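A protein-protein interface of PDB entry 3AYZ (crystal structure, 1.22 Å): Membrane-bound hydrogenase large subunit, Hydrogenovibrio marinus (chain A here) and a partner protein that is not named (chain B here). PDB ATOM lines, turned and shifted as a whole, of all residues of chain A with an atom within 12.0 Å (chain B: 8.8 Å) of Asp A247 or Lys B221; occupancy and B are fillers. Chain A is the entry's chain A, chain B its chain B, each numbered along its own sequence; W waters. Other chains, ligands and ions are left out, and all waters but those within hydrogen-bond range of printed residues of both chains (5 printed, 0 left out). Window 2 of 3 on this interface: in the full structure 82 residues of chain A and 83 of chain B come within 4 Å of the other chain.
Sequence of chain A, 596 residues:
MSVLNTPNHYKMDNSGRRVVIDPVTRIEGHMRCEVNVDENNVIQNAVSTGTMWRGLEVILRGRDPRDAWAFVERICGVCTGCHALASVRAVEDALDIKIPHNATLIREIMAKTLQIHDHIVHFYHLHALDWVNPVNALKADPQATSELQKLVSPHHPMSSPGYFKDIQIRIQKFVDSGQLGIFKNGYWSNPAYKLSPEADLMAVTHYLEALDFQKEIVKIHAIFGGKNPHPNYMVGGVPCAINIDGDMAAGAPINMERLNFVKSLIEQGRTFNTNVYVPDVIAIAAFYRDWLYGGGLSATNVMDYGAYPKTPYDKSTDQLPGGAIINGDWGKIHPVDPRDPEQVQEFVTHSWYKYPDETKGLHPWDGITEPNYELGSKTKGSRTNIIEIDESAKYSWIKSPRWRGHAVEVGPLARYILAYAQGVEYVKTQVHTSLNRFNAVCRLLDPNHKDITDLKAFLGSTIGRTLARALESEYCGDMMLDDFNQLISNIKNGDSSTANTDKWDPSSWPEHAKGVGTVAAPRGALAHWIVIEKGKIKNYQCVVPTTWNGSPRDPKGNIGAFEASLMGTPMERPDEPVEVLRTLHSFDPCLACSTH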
ATOM      1  N   PRO A 239     -28.755  17.586 -20.384  1.00  0.00           N
ATOM      2  CA  PRO A 239     -27.358  18.041 -20.576  1.00  0.00           C
ATOM      3  C   PRO A 239     -27.169  19.329 -21.347  1.00  0.00           C
ATOM      4  O   PRO A 239     -26.087  19.882 -21.397  1.00  0.00           O
ATOM      5  CB  PRO A 239     -26.655  16.877 -21.321  1.00  0.00           C
ATOM      6  CG  PRO A 239     -27.601  15.764 -21.323  1.00  0.00           C
ATOM      7  CD  PRO A 239     -28.980  16.342 -21.126  1.00  0.00           C
ATOM      8  N   CYS A 240     -28.239  19.744 -22.020  1.00  0.00           N
ATOM      9  CA  CYS A 240     -28.199  20.882 -22.939  1.00  0.00           C
ATOM     10  C   CYS A 240     -28.329  22.200 -22.207  1.00  0.00           C
ATOM     11  O   CYS A 240     -29.359  22.893 -22.181  1.00  0.00           O
ATOM     12  CB  CYS A 240     -29.255  20.690 -24.002  1.00  0.00           C
ATOM     13  SG  CYS A 240     -30.908  20.353 -23.390  1.00  0.00           S
ATOM     14  N   ALA A 241     -27.219  22.590 -21.568  1.00  0.00           N
ATOM     15  CA  ALA A 241     -27.152  23.834 -20.757  1.00  0.00           C
ATOM     16  C   ALA A 241     -27.497  25.046 -21.615  1.00  0.00           C
ATOM     17  O   ALA A 241     -27.176  25.131 -22.787  1.00  0.00           O
ATOM     18  CB  ALA A 241     -25.797  23.938 -20.129  1.00  0.00           C
ATOM     19  N   ILE A 242     -28.140  25.977 -20.942  1.00  0.00           N
ATOM     20  CA  ILE A 242     -28.674  27.206 -21.544  1.00  0.00           C
ATOM     21  C   ILE A 242     -27.848  28.406 -21.201  1.00  0.00           C
ATOM     22  O   ILE A 242     -27.549  28.683 -20.038  1.00  0.00           O
ATOM     23  CB  ILE A 242     -30.129  27.435 -21.076  1.00  0.00           C
ATOM     24  CG1 ILE A 242     -31.060  26.303 -21.459  1.00  0.00           C
ATOM     25  CG2 ILE A 242     -30.699  28.748 -21.602  1.00  0.00           C
ATOM     26  CD1 ILE A 242     -32.371  26.242 -20.734  1.00  0.00           C
ATOM     27  N   ASN A 243     -27.504  29.207 -22.190  1.00  0.00           N
ATOM     28  CA  ASN A 243     -26.817  30.471 -22.020  1.00  0.00           C
ATOM     29  C   ASN A 243     -27.242  31.380 -23.198  1.00  0.00           C
ATOM     30  O   ASN A 243     -26.736  31.194 -24.297  1.00  0.00           O
ATOM     31  CB  ASN A 243     -25.326  30.258 -21.968  1.00  0.00           C
ATOM     32  CG  ASN A 243     -24.501  31.500 -21.813  1.00  0.00           C
ATOM     33  OD1 ASN A 243     -25.057  32.611 -21.668  1.00  0.00           O
ATOM     34  ND2 ASN A 243     -23.190  31.328 -21.786  1.00  0.00           N
ATOM     35  N   ILE A 244     -28.122  32.300 -22.942  1.00  0.00           N
ATOM     36  CA  ILE A 244     -28.646  33.098 -24.006  1.00  0.00           C
ATOM     37  C   ILE A 244     -27.790  34.358 -24.279  1.00  0.00           C
ATOM     38  O   ILE A 244     -27.491  34.709 -25.468  1.00  0.00           O
ATOM     39  CB  ILE A 244     -30.119  33.507 -23.775  1.00  0.00           C
ATOM     40  CG1 ILE A 244     -30.940  32.285 -23.476  1.00  0.00           C
ATOM     41  CG2 ILE A 244     -30.634  34.285 -25.012  1.00  0.00           C
ATOM     42  CD1 ILE A 244     -30.785  31.157 -24.506  1.00  0.00           C
ATOM     43  N   ASP A 245     -27.309  35.029 -23.208  1.00  0.00           N
ATOM     44  CA  ASP A 245     -26.805  36.391 -23.225  1.00  0.00           C
ATOM     45  C   ASP A 245     -25.409  36.501 -22.606  1.00  0.00           C
ATOM     46  O   ASP A 245     -24.943  37.633 -22.526  1.00  0.00           O
ATOM     47  CB  ASP A 245     -27.721  37.379 -22.458  1.00  0.00           C
ATOM     48  CG  ASP A 245     -27.451  38.861 -22.622  1.00  0.00           C
ATOM     49  OD1 ASP A 245     -27.639  39.741 -21.729  1.00  0.00           O
ATOM     50  OD2 ASP A 245     -26.951  39.245 -23.681  1.00  0.00           O
ATOM     51  N   GLY A 246     -24.866  35.459 -22.010  1.00  0.00           N
ATOM     52  CA  GLY A 246     -23.656  35.549 -21.237  1.00  0.00           C
ATOM     53  C   GLY A 246     -22.441  35.212 -21.992  1.00  0.00           C
ATOM     54  O   GLY A 246     -22.408  34.860 -23.212  1.00  0.00           O
ATOM     55  N   ASP A 247     -21.292  35.331 -21.308  1.00  0.00           N
ATOM     56  CA  ASP A 247     -20.005  34.987 -21.868  1.00  0.00           C
ATOM     57  C   ASP A 247     -20.083  33.599 -22.472  1.00  0.00           C
ATOM     58  O   ASP A 247     -20.508  32.636 -21.823  1.00  0.00           O
ATOM     59  CB  ASP A 247     -18.988  35.090 -20.719  1.00  0.00           C
ATOM     60  CG  ASP A 247     -17.527  34.936 -21.020  1.00  0.00           C
ATOM     61  OD1 ASP A 247     -16.817  34.302 -20.223  1.00  0.00           O
ATOM     62  OD2 ASP A 247     -17.148  35.497 -22.060  1.00  0.00           O
ATOM     63  N   MET A 248     -19.588  33.476 -23.700  1.00  0.00           N
ATOM     64  CA  MET A 248     -19.462  32.198 -24.419  1.00  0.00           C
ATOM     65  C   MET A 248     -20.807  31.621 -24.828  1.00  0.00           C
ATOM     66  O   MET A 248     -20.871  30.436 -25.121  1.00  0.00           O
ATOM     67  CB  MET A 248     -18.666  31.176 -23.645  1.00  0.00           C
ATOM     68  CG  MET A 248     -17.454  31.805 -22.877  1.00  0.00           C
ATOM     69  SD  MET A 248     -16.406  32.170 -24.221  1.00  0.00           S
ATOM     70  CE  MET A 248     -15.823  30.385 -23.884  1.00  0.00           C
ATOM     71  N   ALA A 249     -21.872  32.368 -24.897  1.00  0.00           N
ATOM     72  CA  ALA A 249     -23.210  31.824 -25.255  1.00  0.00           C
ATOM     73  C   ALA A 249     -23.205  31.071 -26.541  1.00  0.00           C
ATOM     74  O   ALA A 249     -23.876  30.010 -26.653  1.00  0.00           O
ATOM     75  CB  ALA A 249     -24.229  32.971 -25.324  1.00  0.00           C
ATOM     76  N   ALA A 250     -22.476  31.534 -27.565  1.00  0.00           N
ATOM     77  CA  ALA A 250     -22.470  30.809 -28.847  1.00  0.00           C
ATOM     78  C   ALA A 250     -21.977  29.397 -28.702  1.00  0.00           C
ATOM     79  O   ALA A 250     -22.339  28.559 -29.510  1.00  0.00           O
ATOM     80  CB  ALA A 250     -21.686  31.616 -29.865  1.00  0.00           C
ATOM     81  N   GLY A 251     -21.127  29.137 -27.731  1.00  0.00           N
ATOM     82  CA  GLY A 251     -20.650  27.798 -27.437  1.00  0.00           C
ATOM     83  C   GLY A 251     -21.453  26.961 -26.524  1.00  0.00           C
ATOM     84  O   GLY A 251     -21.150  25.766 -26.315  1.00  0.00           O
ATOM     85  N   ALA A 252     -22.544  27.501 -25.941  1.00  0.00           N
ATOM     86  CA  ALA A 252     -23.445  26.711 -25.113  1.00  0.00           C
ATOM     87  C   ALA A 252     -24.360  25.827 -25.947  1.00  0.00           C
ATOM     88  O   ALA A 252     -24.695  26.184 -27.065  1.00  0.00           O
ATOM     89  CB  ALA A 252     -24.340  27.603 -24.262  1.00  0.00           C
ATOM     90  N   PRO A 253     -24.790  24.662 -25.398  1.00  0.00           N
ATOM     91  CA  PRO A 253     -25.776  23.850 -26.130  1.00  0.00           C
ATOM     92  C   PRO A 253     -26.980  24.647 -26.568  1.00  0.00           C
ATOM     93  O   PRO A 253     -27.375  24.536 -27.742  1.00  0.00           O
ATOM     94  CB  PRO A 253     -26.108  22.779 -25.116  1.00  0.00           C
ATOM     95  CG  PRO A 253     -24.844  22.567 -24.358  1.00  0.00           C
ATOM     96  CD  PRO A 253     -24.308  23.985 -24.213  1.00  0.00           C
ATOM     97  N   ILE A 254     -27.577  25.465 -25.692  1.00  0.00           N
ATOM     98  CA  ILE A 254     -28.773  26.191 -26.036  1.00  0.00           C
ATOM     99  C   ILE A 254     -28.487  27.680 -25.906  1.00  0.00           C
ATOM    100  O   ILE A 254     -28.192  28.195 -24.814  1.00  0.00           O
ATOM    101  CB  ILE A 254     -29.955  25.769 -25.176  1.00  0.00           C
ATOM    102  CG1 ILE A 254     -30.204  24.255 -25.277  1.00  0.00           C
ATOM    103  CG2 ILE A 254     -31.237  26.537 -25.476  1.00  0.00           C
ATOM    104  CD1 ILE A 254     -30.586  23.729 -26.642  1.00  0.00           C
ATOM    105  N   ASN A 255     -28.645  28.380 -26.985  1.00  0.00           N
ATOM    106  CA  ASN A 255     -28.439  29.824 -27.093  1.00  0.00           C
ATOM    107  C   ASN A 255     -29.568  30.394 -27.914  1.00  0.00           C
ATOM    108  O   ASN A 255     -30.514  29.701 -28.290  1.00  0.00           O
ATOM    109  CB  ASN A 255     -27.038  30.122 -27.601  1.00  0.00           C
ATOM    110  CG  ASN A 255     -26.813  29.494 -28.948  1.00  0.00           C
ATOM    111  OD1 ASN A 255     -27.692  29.571 -29.837  1.00  0.00           O
ATOM    112  ND2 ASN A 255     -25.740  28.837 -29.172  1.00  0.00           N
ATOM    113  N   MET A 256     -29.548  31.700 -28.218  1.00  0.00           N
ATOM    114  CA  MET A 256     -30.654  32.311 -28.934  1.00  0.00           C
ATOM    115  C   MET A 256     -30.908  31.644 -30.263  1.00  0.00           C
ATOM    116  O   MET A 256     -32.051  31.481 -30.696  1.00  0.00           O
ATOM    117  CB  MET A 256     -30.391  33.814 -29.127  1.00  0.00           C
ATOM    118  CG  MET A 256     -31.610  34.537 -29.693  1.00  0.00           C
ATOM    119  SD  MET A 256     -32.864  34.859 -28.496  1.00  0.00           S
ATOM    120  CE  MET A 256     -34.232  33.888 -28.921  1.00  0.00           C
ATOM    121  N   ARG A 258     -30.246  28.614 -31.282  1.00  0.00           N
ATOM    122  CA  ARG A 258     -30.809  27.280 -31.140  1.00  0.00           C
ATOM    123  C   ARG A 258     -32.276  27.376 -30.800  1.00  0.00           C
ATOM    124  O   ARG A 258     -33.099  26.586 -31.296  1.00  0.00           O
ATOM    125  CB  ARG A 258     -30.034  26.478 -30.092  1.00  0.00           C
ATOM    126  CG  ARG A 258     -28.566  26.221 -30.358  1.00  0.00           C
ATOM    127  CD  ARG A 258     -28.296  25.022 -31.325  1.00  0.00           C
ATOM    128  NE  ARG A 258     -28.405  25.445 -32.668  1.00  0.00           N
ATOM    129  CZ  ARG A 258     -28.049  24.672 -33.716  1.00  0.00           C
ATOM    130  NH1 ARG A 258     -28.098  25.183 -34.938  1.00  0.00           N
ATOM    131  NH2 ARG A 258     -27.734  23.453 -33.455  1.00  0.00           N
ATOM    132  N   SER A 496     -32.499  29.821 -16.238  1.00  0.00           N
ATOM    133  CA  SER A 496     -31.852  29.079 -17.312  1.00  0.00           C
ATOM    134  C   SER A 496     -31.346  27.728 -16.813  1.00  0.00           C
ATOM    135  O   SER A 496     -30.642  27.045 -17.548  1.00  0.00           O
ATOM    136  CB  SER A 496     -30.747  29.857 -17.917  1.00  0.00           C
ATOM    137  OG  SER A 496     -31.161  30.969 -18.657  1.00  0.00           O
ATOM    138  N   THR A 498     -30.856  23.830 -15.788  1.00  0.00           N
ATOM    139  CA  THR A 498     -31.178  22.592 -16.482  1.00  0.00           C
ATOM    140  C   THR A 498     -30.867  21.325 -15.700  1.00  0.00           C
ATOM    141  O   THR A 498     -31.276  20.247 -16.158  1.00  0.00           O
ATOM    142  CB  THR A 498     -30.510  22.515 -17.878  1.00  0.00           C
ATOM    143  OG1 THR A 498     -29.110  22.847 -17.710  1.00  0.00           O
ATOM    144  CG2 THR A 498     -31.154  23.411 -18.891  1.00  0.00           C
ATOM    145  N   TYR B 200     -14.584  20.638 -31.705  1.00  0.00           N
ATOM    146  CA  TYR B 200     -14.569  22.110 -31.484  1.00  0.00           C
ATOM    147  C   TYR B 200     -14.440  22.478 -29.989  1.00  0.00           C
ATOM    148  O   TYR B 200     -14.099  23.624 -29.755  1.00  0.00           O
ATOM    149  CB  TYR B 200     -15.843  22.725 -32.136  1.00  0.00           C
ATOM    150  CG  TYR B 200     -17.036  22.641 -31.213  1.00  0.00           C
ATOM    151  CD1 TYR B 200     -17.540  23.729 -30.526  1.00  0.00           C
ATOM    152  CD2 TYR B 200     -17.666  21.429 -30.940  1.00  0.00           C
ATOM    153  CE1 TYR B 200     -18.619  23.707 -29.681  1.00  0.00           C
ATOM    154  CE2 TYR B 200     -18.725  21.370 -30.065  1.00  0.00           C
ATOM    155  CZ  TYR B 200     -19.204  22.479 -29.409  1.00  0.00           C
ATOM    156  OH  TYR B 200     -20.224  22.338 -28.495  1.00  0.00           O
ATOM    157  N   ARG B 201     -14.645  21.585 -29.055  1.00  0.00           N
ATOM    158  CA  ARG B 201     -14.375  21.837 -27.644  1.00  0.00           C
ATOM    159  C   ARG B 201     -12.927  21.600 -27.216  1.00  0.00           C
ATOM    160  O   ARG B 201     -12.519  21.825 -26.083  1.00  0.00           O
ATOM    161  CB  ARG B 201     -15.322  21.136 -26.672  1.00  0.00           C
ATOM    162  CG  ARG B 201     -16.792  21.528 -26.907  1.00  0.00           C
ATOM    163  CD  ARG B 201     -17.665  21.021 -25.761  1.00  0.00           C
ATOM    164  NE  ARG B 201     -19.079  21.361 -25.984  1.00  0.00           N
ATOM    165  CZ  ARG B 201     -19.977  21.473 -24.995  1.00  0.00           C
ATOM    166  NH1 ARG B 201     -21.222  21.751 -25.333  1.00  0.00           N
ATOM    167  NH2 ARG B 201     -19.694  21.297 -23.748  1.00  0.00           N
ATOM    168  N   HIS B 204     -10.797  24.002 -25.047  1.00  0.00           N
ATOM    169  CA  HIS B 204     -11.074  23.924 -23.634  1.00  0.00           C
ATOM    170  C   HIS B 204     -10.334  22.759 -22.981  1.00  0.00           C
ATOM    171  O   HIS B 204      -9.711  22.939 -21.939  1.00  0.00           O
ATOM    172  CB  HIS B 204     -12.570  23.872 -23.369  1.00  0.00           C
ATOM    173  CG  HIS B 204     -13.275  25.095 -23.847  1.00  0.00           C
ATOM    174  ND1 HIS B 204     -12.976  26.356 -23.409  1.00  0.00           N
ATOM    175  CD2 HIS B 204     -14.341  25.263 -24.703  1.00  0.00           C
ATOM    176  CE1 HIS B 204     -13.804  27.180 -23.988  1.00  0.00           C
ATOM    177  NE2 HIS B 204     -14.630  26.579 -24.803  1.00  0.00           N
ATOM    178  N   GLN B 209     -10.131  23.424 -19.143  1.00  0.00           N
ATOM    179  CA  GLN B 209     -11.450  24.000 -18.949  1.00  0.00           C
ATOM    180  C   GLN B 209     -12.504  22.964 -19.215  1.00  0.00           C
ATOM    181  O   GLN B 209     -12.763  22.603 -20.353  1.00  0.00           O
ATOM    182  CB  GLN B 209     -11.595  25.210 -19.897  1.00  0.00           C
ATOM    183  CG  GLN B 209     -10.756  26.386 -19.487  1.00  0.00           C
ATOM    184  CD  GLN B 209     -10.712  27.505 -20.513  1.00  0.00           C
ATOM    185  OE1 GLN B 209     -10.990  27.322 -21.666  1.00  0.00           O
ATOM    186  NE2 GLN B 209     -10.291  28.654 -19.991  1.00  0.00           N
ATOM    187  N   PHE B 210     -13.060  22.441 -18.124  1.00  0.00           N
ATOM    188  CA  PHE B 210     -13.961  21.278 -18.155  1.00  0.00           C
ATOM    189  C   PHE B 210     -15.249  21.588 -17.488  1.00  0.00           C
ATOM    190  O   PHE B 210     -15.378  22.392 -16.519  1.00  0.00           O
ATOM    191  CB  PHE B 210     -13.338  20.125 -17.359  1.00  0.00           C
ATOM    192  CG  PHE B 210     -12.010  19.667 -17.912  1.00  0.00           C
ATOM    193  CD1 PHE B 210     -11.930  19.037 -19.144  1.00  0.00           C
ATOM    194  CD2 PHE B 210     -10.846  19.861 -17.217  1.00  0.00           C
ATOM    195  CE1 PHE B 210     -10.782  18.594 -19.666  1.00  0.00           C
ATOM    196  CE2 PHE B 210      -9.632  19.445 -17.707  1.00  0.00           C
ATOM    197  CZ  PHE B 210      -9.596  18.804 -18.962  1.00  0.00           C
ATOM    198  N   VAL B 211     -16.321  20.950 -17.934  1.00  0.00           N
ATOM    199  CA  VAL B 211     -17.525  20.720 -17.122  1.00  0.00           C
ATOM    200  C   VAL B 211     -17.102  19.845 -15.941  1.00  0.00           C
ATOM    201  O   VAL B 211     -16.645  18.724 -16.156  1.00  0.00           O
ATOM    202  CB  VAL B 211     -18.626  20.104 -17.986  1.00  0.00           C
ATOM    203  CG1 VAL B 211     -19.838  19.851 -17.105  1.00  0.00           C
ATOM    204  CG2 VAL B 211     -18.946  20.989 -19.169  1.00  0.00           C
ATOM    205  N   ASP B 215     -24.408  21.461 -15.529  1.00  0.00           N
ATOM    206  CA  ASP B 215     -24.994  22.783 -15.497  1.00  0.00           C
ATOM    207  C   ASP B 215     -24.184  23.734 -14.641  1.00  0.00           C
ATOM    208  O   ASP B 215     -24.714  24.684 -14.095  1.00  0.00           O
ATOM    209  CB  ASP B 215     -26.469  22.775 -15.121  1.00  0.00           C
ATOM    210  CG  ASP B 215     -27.189  24.038 -15.497  1.00  0.00           C
ATOM    211  OD1 ASP B 215     -26.687  24.705 -16.438  1.00  0.00           O
ATOM    212  OD2 ASP B 215     -28.178  24.412 -14.863  1.00  0.00           O
ATOM    213  N   ASP B 216     -22.872  23.518 -14.566  1.00  0.00           N
ATOM    214  CA  ASP B 216     -21.931  24.429 -13.946  1.00  0.00           C
ATOM    215  C   ASP B 216     -21.525  25.542 -14.922  1.00  0.00           C
ATOM    216  O   ASP B 216     -22.058  25.635 -16.039  1.00  0.00           O
ATOM    217  CB  ASP B 216     -20.742  23.735 -13.313  1.00  0.00           C
ATOM    218  CG  ASP B 216     -19.777  23.088 -14.284  1.00  0.00           C
ATOM    219  OD1 ASP B 216     -19.955  23.197 -15.504  1.00  0.00           O
ATOM    220  OD2 ASP B 216     -18.774  22.522 -13.724  1.00  0.00           O
ATOM    221  N   GLU B 217     -20.602  26.379 -14.449  1.00  0.00           N
ATOM    222  CA  GLU B 217     -20.153  27.473 -15.331  1.00  0.00           C
ATOM    223  C   GLU B 217     -19.637  26.946 -16.646  1.00  0.00           C
ATOM    224  O   GLU B 217     -19.924  27.460 -17.726  1.00  0.00           O
ATOM    225  CB  GLU B 217     -19.062  28.249 -14.611  1.00  0.00           C
ATOM    226  CG  GLU B 217     -18.491  29.358 -15.420  1.00  0.00           C
ATOM    227  CD  GLU B 217     -17.222  29.990 -14.854  1.00  0.00           C
ATOM    228  OE1 GLU B 217     -16.592  30.820 -15.512  1.00  0.00           O
ATOM    229  OE2 GLU B 217     -16.784  29.622 -13.742  1.00  0.00           O
ATOM    230  N   GLY B 218     -18.810  25.887 -16.566  1.00  0.00           N
ATOM    231  CA  GLY B 218     -18.250  25.356 -17.751  1.00  0.00           C
ATOM    232  C   GLY B 218     -19.317  24.790 -18.715  1.00  0.00           C
ATOM    233  O   GLY B 218     -19.185  24.936 -19.936  1.00  0.00           O
ATOM    234  N   ALA B 219     -20.324  24.111 -18.178  1.00  0.00           N
ATOM    235  CA  ALA B 219     -21.380  23.612 -19.041  1.00  0.00           C
ATOM    236  C   ALA B 219     -22.035  24.706 -19.892  1.00  0.00           C
ATOM    237  O   ALA B 219     -22.294  24.539 -21.071  1.00  0.00           O
ATOM    238  CB  ALA B 219     -22.413  22.839 -18.261  1.00  0.00           C
ATOM    239  N   ARG B 220     -22.257  25.848 -19.268  1.00  0.00           N
ATOM    240  CA  ARG B 220     -22.891  26.983 -19.905  1.00  0.00           C
ATOM    241  C   ARG B 220     -22.004  27.758 -20.850  1.00  0.00           C
ATOM    242  O   ARG B 220     -22.509  28.580 -21.596  1.00  0.00           O
ATOM    243  CB  ARG B 220     -23.448  27.917 -18.810  1.00  0.00           C
ATOM    244  CG  ARG B 220     -24.587  27.268 -17.989  1.00  0.00           C
ATOM    245  CD  ARG B 220     -25.013  28.139 -16.842  1.00  0.00           C
ATOM    246  NE  ARG B 220     -26.059  27.488 -16.060  1.00  0.00           N
ATOM    247  CZ  ARG B 220     -26.789  28.060 -15.149  1.00  0.00           C
ATOM    248  NH1 ARG B 220     -26.559  29.364 -14.901  1.00  0.00           N
ATOM    249  NH2 ARG B 220     -27.712  27.371 -14.527  1.00  0.00           N
ATOM    250  N   LYS B 221     -20.707  27.467 -20.811  1.00  0.00           N
ATOM    251  CA  LYS B 221     -19.747  28.040 -21.739  1.00  0.00           C
ATOM    252  C   LYS B 221     -19.342  27.032 -22.826  1.00  0.00           C
ATOM    253  O   LYS B 221     -18.556  27.386 -23.731  1.00  0.00           O
ATOM    254  CB  LYS B 221     -18.503  28.518 -21.012  1.00  0.00           C
ATOM    255  CG  LYS B 221     -18.827  29.719 -20.111  1.00  0.00           C
ATOM    256  CD  LYS B 221     -17.572  30.188 -19.354  1.00  0.00           C
ATOM    257  CE  LYS B 221     -17.897  31.503 -18.614  1.00  0.00           C
ATOM    258  NZ  LYS B 221     -16.702  31.877 -17.838  1.00  0.00           N
ATOM    259  N   GLY B 222     -19.799  25.810 -22.762  1.00  0.00           N
ATOM    260  CA  GLY B 222     -19.381  24.756 -23.676  1.00  0.00           C
ATOM    261  C   GLY B 222     -17.983  24.248 -23.477  1.00  0.00           C
ATOM    262  O   GLY B 222     -17.303  23.847 -24.438  1.00  0.00           O
ATOM    263  N   TYR B 223     -17.555  24.134 -22.215  1.00  0.00           N
ATOM    264  CA  TYR B 223     -16.268  23.559 -21.858  1.00  0.00           C
ATOM    265  C   TYR B 223     -16.209  22.073 -22.174  1.00  0.00           C
ATOM    266  O   TYR B 223     -17.210  21.389 -22.423  1.00  0.00           O
ATOM    267  CB  TYR B 223     -15.955  23.809 -20.393  1.00  0.00           C
ATOM    268  CG  TYR B 223     -15.466  25.180 -20.019  1.00  0.00           C
ATOM    269  CD1 TYR B 223     -15.440  26.246 -20.910  1.00  0.00           C
ATOM    270  CD2 TYR B 223     -15.037  25.418 -18.717  1.00  0.00           C
ATOM    271  CE1 TYR B 223     -14.999  27.482 -20.529  1.00  0.00           C
ATOM    272  CE2 TYR B 223     -14.568  26.674 -18.337  1.00  0.00           C
ATOM    273  CZ  TYR B 223     -14.538  27.714 -19.231  1.00  0.00           C
ATOM    274  OH  TYR B 223     -14.070  28.957 -18.857  1.00  0.00           O
ATOM    275  N   CYS B 224     -15.022  21.500 -22.211  1.00  0.00           N
ATOM    276  CA  CYS B 224     -14.809  20.089 -22.568  1.00  0.00           C
ATOM    277  C   CYS B 224     -15.538  19.170 -21.605  1.00  0.00           C
ATOM    278  O   CYS B 224     -15.616  19.445 -20.397  1.00  0.00           O
ATOM    279  CB  CYS B 224     -13.311  19.816 -22.611  1.00  0.00           C
ATOM    280  SG  CYS B 224     -12.831  18.102 -22.756  1.00  0.00           S
ATOM    281  N   GLN B 253     -21.889  18.673 -28.830  1.00  0.00           N
ATOM    282  CA  GLN B 253     -22.414  20.006 -28.984  1.00  0.00           C
ATOM    283  C   GLN B 253     -23.574  20.248 -28.027  1.00  0.00           C
ATOM    284  O   GLN B 253     -23.686  21.316 -27.410  1.00  0.00           O
ATOM    285  CB  GLN B 253     -22.804  20.290 -30.415  1.00  0.00           C
ATOM    286  CG  GLN B 253     -23.443  21.671 -30.580  1.00  0.00           C
ATOM    287  CD  GLN B 253     -23.700  22.076 -32.029  1.00  0.00           C
ATOM    288  OE1 GLN B 253     -23.262  21.406 -32.957  1.00  0.00           O
ATOM    289  NE2 GLN B 253     -24.330  23.213 -32.180  1.00  0.00           N
HETATM  290  O   HOH W   1     -22.053  23.943 -27.861  1.00  0.00           O
HETATM  291  O   HOH W   2     -17.325  34.536 -17.358  1.00  0.00           O
HETATM  292  O   HOH W   3     -24.936  25.074 -29.856  1.00  0.00           O
HETATM  293  O   HOH W   4     -28.546  25.469 -18.125  1.00  0.00           O
HETATM  294  O   HOH W   5     -27.368  21.853 -31.272  1.00  0.00           O
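The backbone carbonyl oxygen (O) of Ala A241 is in hydrogen-bond range of the backbone NH (N) of Ile A254, at 3.0 Å. The backbone NH (N) of Gly A246 sits at hydrogen-bond distance from the side-chain amide oxygen (OD1) of Asn A243 (2.9 Å). O of Asp A247 is in hydrogen-bond range of ND2 of Asn A243, 3.0 Å away. O of Gln B253 lies within hydrogen-bond range of NH1 of Arg B201, 3.3 Å away. The side-chain amide oxygen (OE1) of Gln B209 is in hydrogen-bond range of a ring nitrogen (ND1) of His B204 (2.8 Å).
Of the 21 printed residues of chain A, 10 touch a printed residue of chain B. Printed residues of chain A that touch a printed residue of chain B: Ala A241, Ile A242, Asn A243, Asp A247, Met A248, Gly A251, Ala A252, Pro A253, Arg A258 and Thr A498. Hydrophobic or aromatic side chains of chain B within 4 Å of the printed part of chain A: His B204. Among the printed residues, 14 pairs touch across the chains. Among the printed residues, Asp or Glu carboxylates within 4 Å of a Lys or Arg side-chain nitrogen of the other chain: Asp A247 with Lys B221 (3.4 Å).
The side-chain amide nitrogen (ND2) of Asn A243 is in hydrogen-bond range of the backbone carbonyl oxygen (O) of Arg B220, 2.8 Å away. The side-chain carboxylate (OD1) of Asp A247 lies within salt-bridge range of the side-chain amino group (NZ) of Lys B221 (3.4 Å). The backbone NH of Thr A498 lies within hydrogen-bond range of the side-chain carboxylate of Asp B215, at 2.9 Å.
Water W1 lies within hydrogen-bond range of OH of Tyr B200, O of Gly A251, O of Gln B253 and NH1 of Arg B201. Water W4 lies within hydrogen-bond range of the side-chain carboxylate of Asp B215, the backbone carbonyl oxygen of Ser A496, the side-chain hydroxyl of Thr A498 and the backbone NH of Ile A242. Water W5 bridges the guanidinium group of Arg A258 (2.7 Å) and the side-chain amide nitrogen of Gln B253 (3.5 Å). Water W2 bridges NZ of Lys B221 (2.8 Å) and OD1 of Asp A247 (2.9 Å).
Among the printed residues, pairs that only touch across the chains: Ala A241 with Asp B215, Ala A241 with Ala B219, Ile A242 with Arg B220, Met A248 with His B204, Met A248 with Lys B221, Gly A251 with Gly B222, Ala A252 with Arg B220, Pro A253 with Arg B201, Pro A253 with Ala B219, Pro A253 with Gln B253 and Arg A258 with Gln B253.
Of the printed residues of chain A, Lys B221 touches Asp A247 (3.4 Å) and Met A248 (3.7 Å). Ala B219 touches just these residues of chain A: Ala A241 and Pro A253. No residue of chain A comes within 4 Å of Tyr B223. Printed residues of chain B within 4 Å of Pro A253: Arg B201 (3.8 Å), Ala B219 (3.8 Å) and Gln B253 (3.5 Å). Of the printed residues of chain A, Asp B215 touches Ala A241 (3.9 Å) and Thr A498 (2.9 Å). Of the printed residues of chain B, Ala A252 touches Arg B220. Of the printed residues of chain B, Asn A243 touches Arg B220. Cys B224 touches none of the printed residues of chain A. The nearest printed residue of chain B that does not touch Asp A247 is Arg B220 (4.5 Å).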
